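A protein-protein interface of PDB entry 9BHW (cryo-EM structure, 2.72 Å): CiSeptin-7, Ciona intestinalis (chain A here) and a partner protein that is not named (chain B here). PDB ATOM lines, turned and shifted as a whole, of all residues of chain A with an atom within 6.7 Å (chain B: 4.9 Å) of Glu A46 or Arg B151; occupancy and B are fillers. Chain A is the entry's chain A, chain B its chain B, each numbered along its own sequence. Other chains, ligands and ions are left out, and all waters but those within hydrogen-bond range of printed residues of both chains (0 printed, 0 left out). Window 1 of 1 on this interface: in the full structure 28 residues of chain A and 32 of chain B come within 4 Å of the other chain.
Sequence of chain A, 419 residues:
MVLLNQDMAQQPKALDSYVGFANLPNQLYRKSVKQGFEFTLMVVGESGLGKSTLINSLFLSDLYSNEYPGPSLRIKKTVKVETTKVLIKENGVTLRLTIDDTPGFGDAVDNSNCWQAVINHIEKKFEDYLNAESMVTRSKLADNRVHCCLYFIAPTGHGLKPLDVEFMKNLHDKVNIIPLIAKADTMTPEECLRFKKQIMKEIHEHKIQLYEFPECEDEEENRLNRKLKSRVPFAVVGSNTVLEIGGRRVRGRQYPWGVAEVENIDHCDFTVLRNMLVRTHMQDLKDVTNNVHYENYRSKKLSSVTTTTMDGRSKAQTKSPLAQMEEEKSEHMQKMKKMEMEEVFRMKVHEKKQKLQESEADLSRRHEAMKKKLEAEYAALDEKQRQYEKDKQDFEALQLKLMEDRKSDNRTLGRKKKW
The side-chain carboxylate (OE2) of Glu A46 is in salt-bridge range of the guanidinium group (NH1) of Arg B151 (3.9 Å).
OD1 of Asp A107 is in hydrogen-bond range of N of Ser A47 (3.4 Å).
The side-chain hydroxyl of Ser B36 is in hydrogen-bond range of the guanidinium group of Arg B151, at 2.6 Å.
The backbone carbonyl oxygen (O) of Glu A46 lies within hydrogen-bond range of the side-chain amino group (NZ) of Lys A51, 3.0 Å away.
The side-chain carboxylate of Asp B154 lies within salt-bridge range of the guanidinium group of Arg B151, 3.3 Å away.
Leu B152 touches Asp A107 (CD1 to O, 3.5 Å).
Printed residues of chain B within 4 Å of Glu A46: Arg B151 (3.9 Å).
Of the printed residues of chain A, Arg B151 touches Glu A46.
Of the printed residues of chain A, Leu B152 touches Asp A107.
Printed residues of chain B within 4 Å of Asp A107: Leu B152 (3.5 Å).
Leu A163 touches none of the printed residues of chain B.
The nearest residue of chain A that does not touch Arg B151 is Asp A107 (6.0 Å).
Printed residues of chain A that touch a printed residue of chain B: Glu A46 and Asp A107.
Of the 10 printed residues of chain B, 2 touch a printed residue of chain A.
Printed residues of chain B that touch a printed residue of chain A: Arg B151 and Leu B152.
Hydrophobic or aromatic side chains of chain B that line the printed part of chain A: Leu B152.
Among the printed residues, 2 pairs touch across the chains.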
ATOM      1  N   VAL A  44       5.373  23.482 -12.875  1.00  0.00           N
ATOM      2  CA  VAL A  44       5.689  23.321 -14.287  1.00  0.00           C
ATOM      3  C   VAL A  44       4.401  23.449 -15.084  1.00  0.00           C
ATOM      4  O   VAL A  44       3.401  22.792 -14.768  1.00  0.00           O
ATOM      5  CB  VAL A  44       6.364  21.967 -14.566  1.00  0.00           C
ATOM      6  CG1 VAL A  44       6.649  21.813 -16.046  1.00  0.00           C
ATOM      7  CG2 VAL A  44       7.631  21.822 -13.747  1.00  0.00           C
ATOM      8  N   GLY A  45       4.423  24.299 -16.103  1.00  0.00           N
ATOM      9  CA  GLY A  45       3.290  24.445 -16.989  1.00  0.00           C
ATOM     10  C   GLY A  45       3.431  25.615 -17.933  1.00  0.00           C
ATOM     11  O   GLY A  45       4.278  26.489 -17.729  1.00  0.00           O
ATOM     12  N   GLU A  46       2.610  25.644 -18.975  1.00  0.00           N
ATOM     13  CA  GLU A  46       2.598  26.774 -19.889  1.00  0.00           C
ATOM     14  C   GLU A  46       2.041  28.009 -19.193  1.00  0.00           C
ATOM     15  O   GLU A  46       1.286  27.915 -18.223  1.00  0.00           O
ATOM     16  CB  GLU A  46       1.774  26.443 -21.131  1.00  0.00           C
ATOM     17  CG  GLU A  46       2.287  27.076 -22.408  1.00  0.00           C
ATOM     18  CD  GLU A  46       1.514  26.622 -23.630  1.00  0.00           C
ATOM     19  OE1 GLU A  46       0.518  25.887 -23.464  1.00  0.00           O
ATOM     20  OE2 GLU A  46       1.899  27.000 -24.756  1.00  0.00           O
ATOM     21  N   SER A  47       2.431  29.176 -19.692  1.00  0.00           N
ATOM     22  CA  SER A  47       2.053  30.429 -19.057  1.00  0.00           C
ATOM     23  C   SER A  47       0.561  30.689 -19.197  1.00  0.00           C
ATOM     24  O   SER A  47      -0.077  30.280 -20.169  1.00  0.00           O
ATOM     25  CB  SER A  47       2.841  31.588 -19.661  1.00  0.00           C
ATOM     26  OG  SER A  47       2.463  32.820 -19.075  1.00  0.00           O
ATOM     27  N   GLY A  48       0.001  31.383 -18.208  1.00  0.00           N
ATOM     28  CA  GLY A  48      -1.409  31.709 -18.248  1.00  0.00           C
ATOM     29  C   GLY A  48      -2.337  30.570 -17.901  1.00  0.00           C
ATOM     30  O   GLY A  48      -3.447  30.502 -18.435  1.00  0.00           O
ATOM     31  N   LEU A  49      -1.911  29.663 -17.021  1.00  0.00           N
ATOM     32  CA  LEU A  49      -2.723  28.530 -16.602  1.00  0.00           C
ATOM     33  C   LEU A  49      -3.109  28.606 -15.129  1.00  0.00           C
ATOM     34  O   LEU A  49      -3.464  27.586 -14.533  1.00  0.00           O
ATOM     35  CB  LEU A  49      -1.994  27.221 -16.896  1.00  0.00           C
ATOM     36  CG  LEU A  49      -1.922  26.784 -18.360  1.00  0.00           C
ATOM     37  CD1 LEU A  49      -1.232  25.445 -18.485  1.00  0.00           C
ATOM     38  CD2 LEU A  49      -3.303  26.722 -18.972  1.00  0.00           C
ATOM     39  N   GLY A  50      -3.051  29.789 -14.529  1.00  0.00           N
ATOM     40  CA  GLY A  50      -3.458  29.946 -13.146  1.00  0.00           C
ATOM     41  C   GLY A  50      -2.485  29.403 -12.126  1.00  0.00           C
ATOM     42  O   GLY A  50      -2.893  29.063 -11.012  1.00  0.00           O
ATOM     43  N   LYS A  51      -1.218  29.335 -12.497  1.00  0.00           N
ATOM     44  CA  LYS A  51      -0.201  28.732 -11.625  1.00  0.00           C
ATOM     45  C   LYS A  51       0.027  29.604 -10.408  1.00  0.00           C
ATOM     46  O   LYS A  51      -0.097  29.080  -9.308  1.00  0.00           O
ATOM     47  CB  LYS A  51       1.043  28.375 -12.435  1.00  0.00           C
ATOM     48  CG  LYS A  51       0.793  27.605 -13.718  1.00  0.00           C
ATOM     49  CD  LYS A  51       2.069  27.163 -14.373  1.00  0.00           C
ATOM     50  CE  LYS A  51       2.982  28.315 -14.712  1.00  0.00           C
ATOM     51  NZ  LYS A  51       2.377  29.202 -15.730  1.00  0.00           N
ATOM     52  N   GLY A 104       8.816  30.245 -18.722  1.00  0.00           N
ATOM     53  CA  GLY A 104       9.206  30.013 -20.092  1.00  0.00           C
ATOM     54  C   GLY A 104       8.947  28.615 -20.602  1.00  0.00           C
ATOM     55  O   GLY A 104       9.292  28.323 -21.753  1.00  0.00           O
ATOM     56  N   PHE A 105       8.350  27.746 -19.796  1.00  0.00           N
ATOM     57  CA  PHE A 105       8.071  26.385 -20.232  1.00  0.00           C
ATOM     58  C   PHE A 105       6.926  26.385 -21.234  1.00  0.00           C
ATOM     59  O   PHE A 105       5.832  26.876 -20.939  1.00  0.00           O
ATOM     60  CB  PHE A 105       7.731  25.507 -19.031  1.00  0.00           C
ATOM     61  CG  PHE A 105       7.609  24.053 -19.363  1.00  0.00           C
ATOM     62  CD1 PHE A 105       8.716  23.231 -19.331  1.00  0.00           C
ATOM     63  CD2 PHE A 105       6.389  23.506 -19.705  1.00  0.00           C
ATOM     64  CE1 PHE A 105       8.607  21.895 -19.637  1.00  0.00           C
ATOM     65  CE2 PHE A 105       6.276  22.173 -20.012  1.00  0.00           C
ATOM     66  CZ  PHE A 105       7.388  21.366 -19.978  1.00  0.00           C
ATOM     67  N   GLY A 106       7.177  25.836 -22.418  1.00  0.00           N
ATOM     68  CA  GLY A 106       6.147  25.733 -23.428  1.00  0.00           C
ATOM     69  C   GLY A 106       5.767  27.031 -24.095  1.00  0.00           C
ATOM     70  O   GLY A 106       4.764  27.069 -24.813  1.00  0.00           O
ATOM     71  N   ASP A 107       6.530  28.098 -23.883  1.00  0.00           N
ATOM     72  CA  ASP A 107       6.229  29.399 -24.458  1.00  0.00           C
ATOM     73  C   ASP A 107       7.002  29.681 -25.736  1.00  0.00           C
ATOM     74  O   ASP A 107       6.908  30.790 -26.267  1.00  0.00           O
ATOM     75  CB  ASP A 107       6.511  30.500 -23.436  1.00  0.00           C
ATOM     76  CG  ASP A 107       5.510  30.509 -22.303  1.00  0.00           C
ATOM     77  OD1 ASP A 107       4.689  29.573 -22.228  1.00  0.00           O
ATOM     78  OD2 ASP A 107       5.544  31.451 -21.485  1.00  0.00           O
ATOM     79  N   ALA A 108       7.758  28.715 -26.240  1.00  0.00           N
ATOM     80  CA  ALA A 108       8.577  28.901 -27.425  1.00  0.00           C
ATOM     81  C   ALA A 108       7.977  28.165 -28.612  1.00  0.00           C
ATOM     82  O   ALA A 108       7.169  27.246 -28.461  1.00  0.00           O
ATOM     83  CB  ALA A 108      10.006  28.417 -27.177  1.00  0.00           C
ATOM     84  N   ASN A 111      10.017  23.612 -28.814  1.00  0.00           N
ATOM     85  CA  ASN A 111      10.125  23.216 -27.417  1.00  0.00           C
ATOM     86  C   ASN A 111      10.920  21.930 -27.240  1.00  0.00           C
ATOM     87  O   ASN A 111      10.740  21.228 -26.242  1.00  0.00           O
ATOM     88  CB  ASN A 111       8.735  23.070 -26.803  1.00  0.00           C
ATOM     89  CG  ASN A 111       8.137  24.395 -26.401  1.00  0.00           C
ATOM     90  OD1 ASN A 111       8.755  25.169 -25.675  1.00  0.00           O
ATOM     91  ND2 ASN A 111       6.926  24.664 -26.867  1.00  0.00           N
ATOM     92  N   TYR A 151       2.376  19.602 -12.222  1.00  0.00           N
ATOM     93  CA  TYR A 151       2.324  19.802 -13.662  1.00  0.00           C
ATOM     94  C   TYR A 151       0.927  20.250 -14.060  1.00  0.00           C
ATOM     95  O   TYR A 151      -0.063  19.615 -13.684  1.00  0.00           O
ATOM     96  CB  TYR A 151       2.694  18.531 -14.421  1.00  0.00           C
ATOM     97  CG  TYR A 151       2.892  18.784 -15.891  1.00  0.00           C
ATOM     98  CD1 TYR A 151       3.987  19.495 -16.345  1.00  0.00           C
ATOM     99  CD2 TYR A 151       1.969  18.348 -16.822  1.00  0.00           C
ATOM    100  CE1 TYR A 151       4.169  19.745 -17.681  1.00  0.00           C
ATOM    101  CE2 TYR A 151       2.144  18.595 -18.163  1.00  0.00           C
ATOM    102  CZ  TYR A 151       3.246  19.295 -18.585  1.00  0.00           C
ATOM    103  OH  TYR A 151       3.430  19.547 -19.923  1.00  0.00           O
ATOM    104  N   PHE A 152       0.850  21.333 -14.820  1.00  0.00           N
ATOM    105  CA  PHE A 152      -0.422  21.894 -15.247  1.00  0.00           C
ATOM    106  C   PHE A 152      -0.698  21.492 -16.690  1.00  0.00           C
ATOM    107  O   PHE A 152       0.104  21.779 -17.584  1.00  0.00           O
ATOM    108  CB  PHE A 152      -0.421  23.412 -15.096  1.00  0.00           C
ATOM    109  CG  PHE A 152      -0.521  23.877 -13.677  1.00  0.00           C
ATOM    110  CD1 PHE A 152       0.529  23.703 -12.801  1.00  0.00           C
ATOM    111  CD2 PHE A 152      -1.665  24.490 -13.218  1.00  0.00           C
ATOM    112  CE1 PHE A 152       0.435  24.134 -11.499  1.00  0.00           C
ATOM    113  CE2 PHE A 152      -1.758  24.917 -11.918  1.00  0.00           C
ATOM    114  CZ  PHE A 152      -0.709  24.738 -11.061  1.00  0.00           C
ATOM    115  N   ALA A 154      -3.251  21.792 -19.949  1.00  0.00           N
ATOM    116  CA  ALA A 154      -4.201  22.762 -20.468  1.00  0.00           C
ATOM    117  C   ALA A 154      -5.589  22.138 -20.581  1.00  0.00           C
ATOM    118  O   ALA A 154      -5.724  20.995 -21.027  1.00  0.00           O
ATOM    119  CB  ALA A 154      -3.749  23.279 -21.830  1.00  0.00           C
ATOM    120  N   LYS A 161      -0.941  16.350 -24.701  1.00  0.00           N
ATOM    121  CA  LYS A 161      -0.121  16.818 -25.797  1.00  0.00           C
ATOM    122  C   LYS A 161       1.208  16.067 -25.794  1.00  0.00           C
ATOM    123  O   LYS A 161       1.607  15.501 -24.774  1.00  0.00           O
ATOM    124  CB  LYS A 161       0.120  18.319 -25.675  1.00  0.00           C
ATOM    125  CG  LYS A 161      -1.119  19.179 -25.843  1.00  0.00           C
ATOM    126  CD  LYS A 161      -1.945  18.740 -27.035  1.00  0.00           C
ATOM    127  CE  LYS A 161      -3.061  19.730 -27.322  1.00  0.00           C
ATOM    128  NZ  LYS A 161      -2.542  21.012 -27.871  1.00  0.00           N
ATOM    129  N   LEU A 163       4.135  17.303 -25.697  1.00  0.00           N
ATOM    130  CA  LEU A 163       5.056  17.924 -24.750  1.00  0.00           C
ATOM    131  C   LEU A 163       4.843  17.398 -23.336  1.00  0.00           C
ATOM    132  O   LEU A 163       5.811  17.111 -22.619  1.00  0.00           O
ATOM    133  CB  LEU A 163       4.899  19.441 -24.786  1.00  0.00           C
ATOM    134  CG  LEU A 163       5.772  20.244 -23.825  1.00  0.00           C
ATOM    135  CD1 LEU A 163       7.228  19.896 -24.015  1.00  0.00           C
ATOM    136  CD2 LEU A 163       5.551  21.726 -24.027  1.00  0.00           C
ATOM    137  N   SER B  36      -4.791  25.857 -32.167  1.00  0.00           N
ATOM    138  CA  SER B  36      -4.367  24.645 -31.484  1.00  0.00           C
ATOM    139  C   SER B  36      -5.558  23.737 -31.213  1.00  0.00           C
ATOM    140  O   SER B  36      -6.701  24.188 -31.101  1.00  0.00           O
ATOM    141  CB  SER B  36      -3.665  24.986 -30.175  1.00  0.00           C
ATOM    142  OG  SER B  36      -2.525  25.790 -30.408  1.00  0.00           O
ATOM    143  N   GLY B  95       0.338  23.652 -33.905  1.00  0.00           N
ATOM    144  CA  GLY B  95       0.685  24.190 -32.607  1.00  0.00           C
ATOM    145  C   GLY B  95       0.667  23.203 -31.466  1.00  0.00           C
ATOM    146  O   GLY B  95       0.644  23.623 -30.307  1.00  0.00           O
ATOM    147  N   PRO B 144      -5.946  31.122 -27.640  1.00  0.00           N
ATOM    148  CA  PRO B 144      -6.235  30.539 -26.333  1.00  0.00           C
ATOM    149  C   PRO B 144      -6.421  31.614 -25.281  1.00  0.00           C
ATOM    150  O   PRO B 144      -5.737  32.648 -25.305  1.00  0.00           O
ATOM    151  CB  PRO B 144      -4.993  29.680 -26.046  1.00  0.00           C
ATOM    152  CG  PRO B 144      -3.987  30.075 -27.062  1.00  0.00           C
ATOM    153  CD  PRO B 144      -4.749  30.529 -28.247  1.00  0.00           C
ATOM    154  N   SER B 149      -1.145  37.491 -22.874  1.00  0.00           N
ATOM    155  CA  SER B 149      -0.706  38.033 -24.154  1.00  0.00           C
ATOM    156  C   SER B 149      -0.813  36.925 -25.191  1.00  0.00           C
ATOM    157  O   SER B 149      -1.138  35.778 -24.870  1.00  0.00           O
ATOM    158  CB  SER B 149       0.720  38.573 -24.077  1.00  0.00           C
ATOM    159  OG  SER B 149       1.659  37.513 -24.115  1.00  0.00           O
ATOM    160  N   LEU B 150      -0.532  37.275 -26.441  1.00  0.00           N
ATOM    161  CA  LEU B 150      -0.552  36.288 -27.508  1.00  0.00           C
ATOM    162  C   LEU B 150       0.675  35.393 -27.419  1.00  0.00           C
ATOM    163  O   LEU B 150       1.738  35.810 -26.951  1.00  0.00           O
ATOM    164  CB  LEU B 150      -0.594  36.961 -28.877  1.00  0.00           C
ATOM    165  CG  LEU B 150      -1.905  37.543 -29.399  1.00  0.00           C
ATOM    166  CD1 LEU B 150      -2.259  38.794 -28.635  1.00  0.00           C
ATOM    167  CD2 LEU B 150      -1.806  37.842 -30.875  1.00  0.00           C
ATOM    168  N   ARG B 151       0.522  34.155 -27.864  1.00  0.00           N
ATOM    169  CA  ARG B 151       1.660  33.262 -27.963  1.00  0.00           C
ATOM    170  C   ARG B 151       2.521  33.639 -29.162  1.00  0.00           C
ATOM    171  O   ARG B 151       2.089  34.348 -30.076  1.00  0.00           O
ATOM    172  CB  ARG B 151       1.198  31.814 -28.084  1.00  0.00           C
ATOM    173  CG  ARG B 151       0.166  31.413 -27.067  1.00  0.00           C
ATOM    174  CD  ARG B 151      -0.059  29.917 -27.087  1.00  0.00           C
ATOM    175  NE  ARG B 151      -0.454  29.438 -28.404  1.00  0.00           N
ATOM    176  CZ  ARG B 151      -0.700  28.169 -28.694  1.00  0.00           C
ATOM    177  NH1 ARG B 151      -0.588  27.220 -27.782  1.00  0.00           N
ATOM    178  NH2 ARG B 151      -1.069  27.845 -29.928  1.00  0.00           N
ATOM    179  N   LEU B 152       3.762  33.155 -29.150  1.00  0.00           N
ATOM    180  CA  LEU B 152       4.675  33.455 -30.246  1.00  0.00           C
ATOM    181  C   LEU B 152       4.214  32.801 -31.541  1.00  0.00           C
ATOM    182  O   LEU B 152       4.284  33.414 -32.617  1.00  0.00           O
ATOM    183  CB  LEU B 152       6.088  33.009 -29.880  1.00  0.00           C
ATOM    184  CG  LEU B 152       6.662  33.595 -28.587  1.00  0.00           C
ATOM    185  CD1 LEU B 152       8.127  33.229 -28.436  1.00  0.00           C
ATOM    186  CD2 LEU B 152       6.482  35.096 -28.546  1.00  0.00           C
ATOM    187  N   VAL B 153       3.730  31.562 -31.456  1.00  0.00           N
ATOM    188  CA  VAL B 153       3.251  30.861 -32.644  1.00  0.00           C
ATOM    189  C   VAL B 153       2.071  31.603 -33.255  1.00  0.00           C
ATOM    190  O   VAL B 153       1.948  31.704 -34.482  1.00  0.00           O
ATOM    191  CB  VAL B 153       2.888  29.408 -32.297  1.00  0.00           C
ATOM    192  CG1 VAL B 153       2.585  28.627 -33.551  1.00  0.00           C
ATOM    193  CG2 VAL B 153       4.014  28.756 -31.529  1.00  0.00           C
ATOM    194  N   ASP B 154       1.190  32.137 -32.408  1.00  0.00           N
ATOM    195  CA  ASP B 154       0.039  32.881 -32.908  1.00  0.00           C
ATOM    196  C   ASP B 154       0.470  34.126 -33.667  1.00  0.00           C
ATOM    197  O   ASP B 154      -0.048  34.408 -34.754  1.00  0.00           O
ATOM    198  CB  ASP B 154      -0.888  33.246 -31.752  1.00  0.00           C
ATOM    199  CG  ASP B 154      -1.521  32.030 -31.110  1.00  0.00           C
ATOM    200  OD1 ASP B 154      -1.781  31.046 -31.830  1.00  0.00           O
ATOM    201  OD2 ASP B 154      -1.759  32.058 -29.886  1.00  0.00           O
ATOM    202  N   ILE B 155       1.427  34.876 -33.121  1.00  0.00           N
ATOM    203  CA  ILE B 155       1.922  36.070 -33.800  1.00  0.00           C
ATOM    204  C   ILE B 155       2.534  35.699 -35.145  1.00  0.00           C
ATOM    205  O   ILE B 155       2.236  36.320 -36.175  1.00  0.00           O
ATOM    206  CB  ILE B 155       2.932  36.812 -32.912  1.00  0.00           C
ATOM    207  CG1 ILE B 155       2.228  37.440 -31.718  1.00  0.00           C
ATOM    208  CG2 ILE B 155       3.662  37.873 -33.711  1.00  0.00           C
ATOM    209  CD1 ILE B 155       3.172  38.020 -30.708  1.00  0.00           C
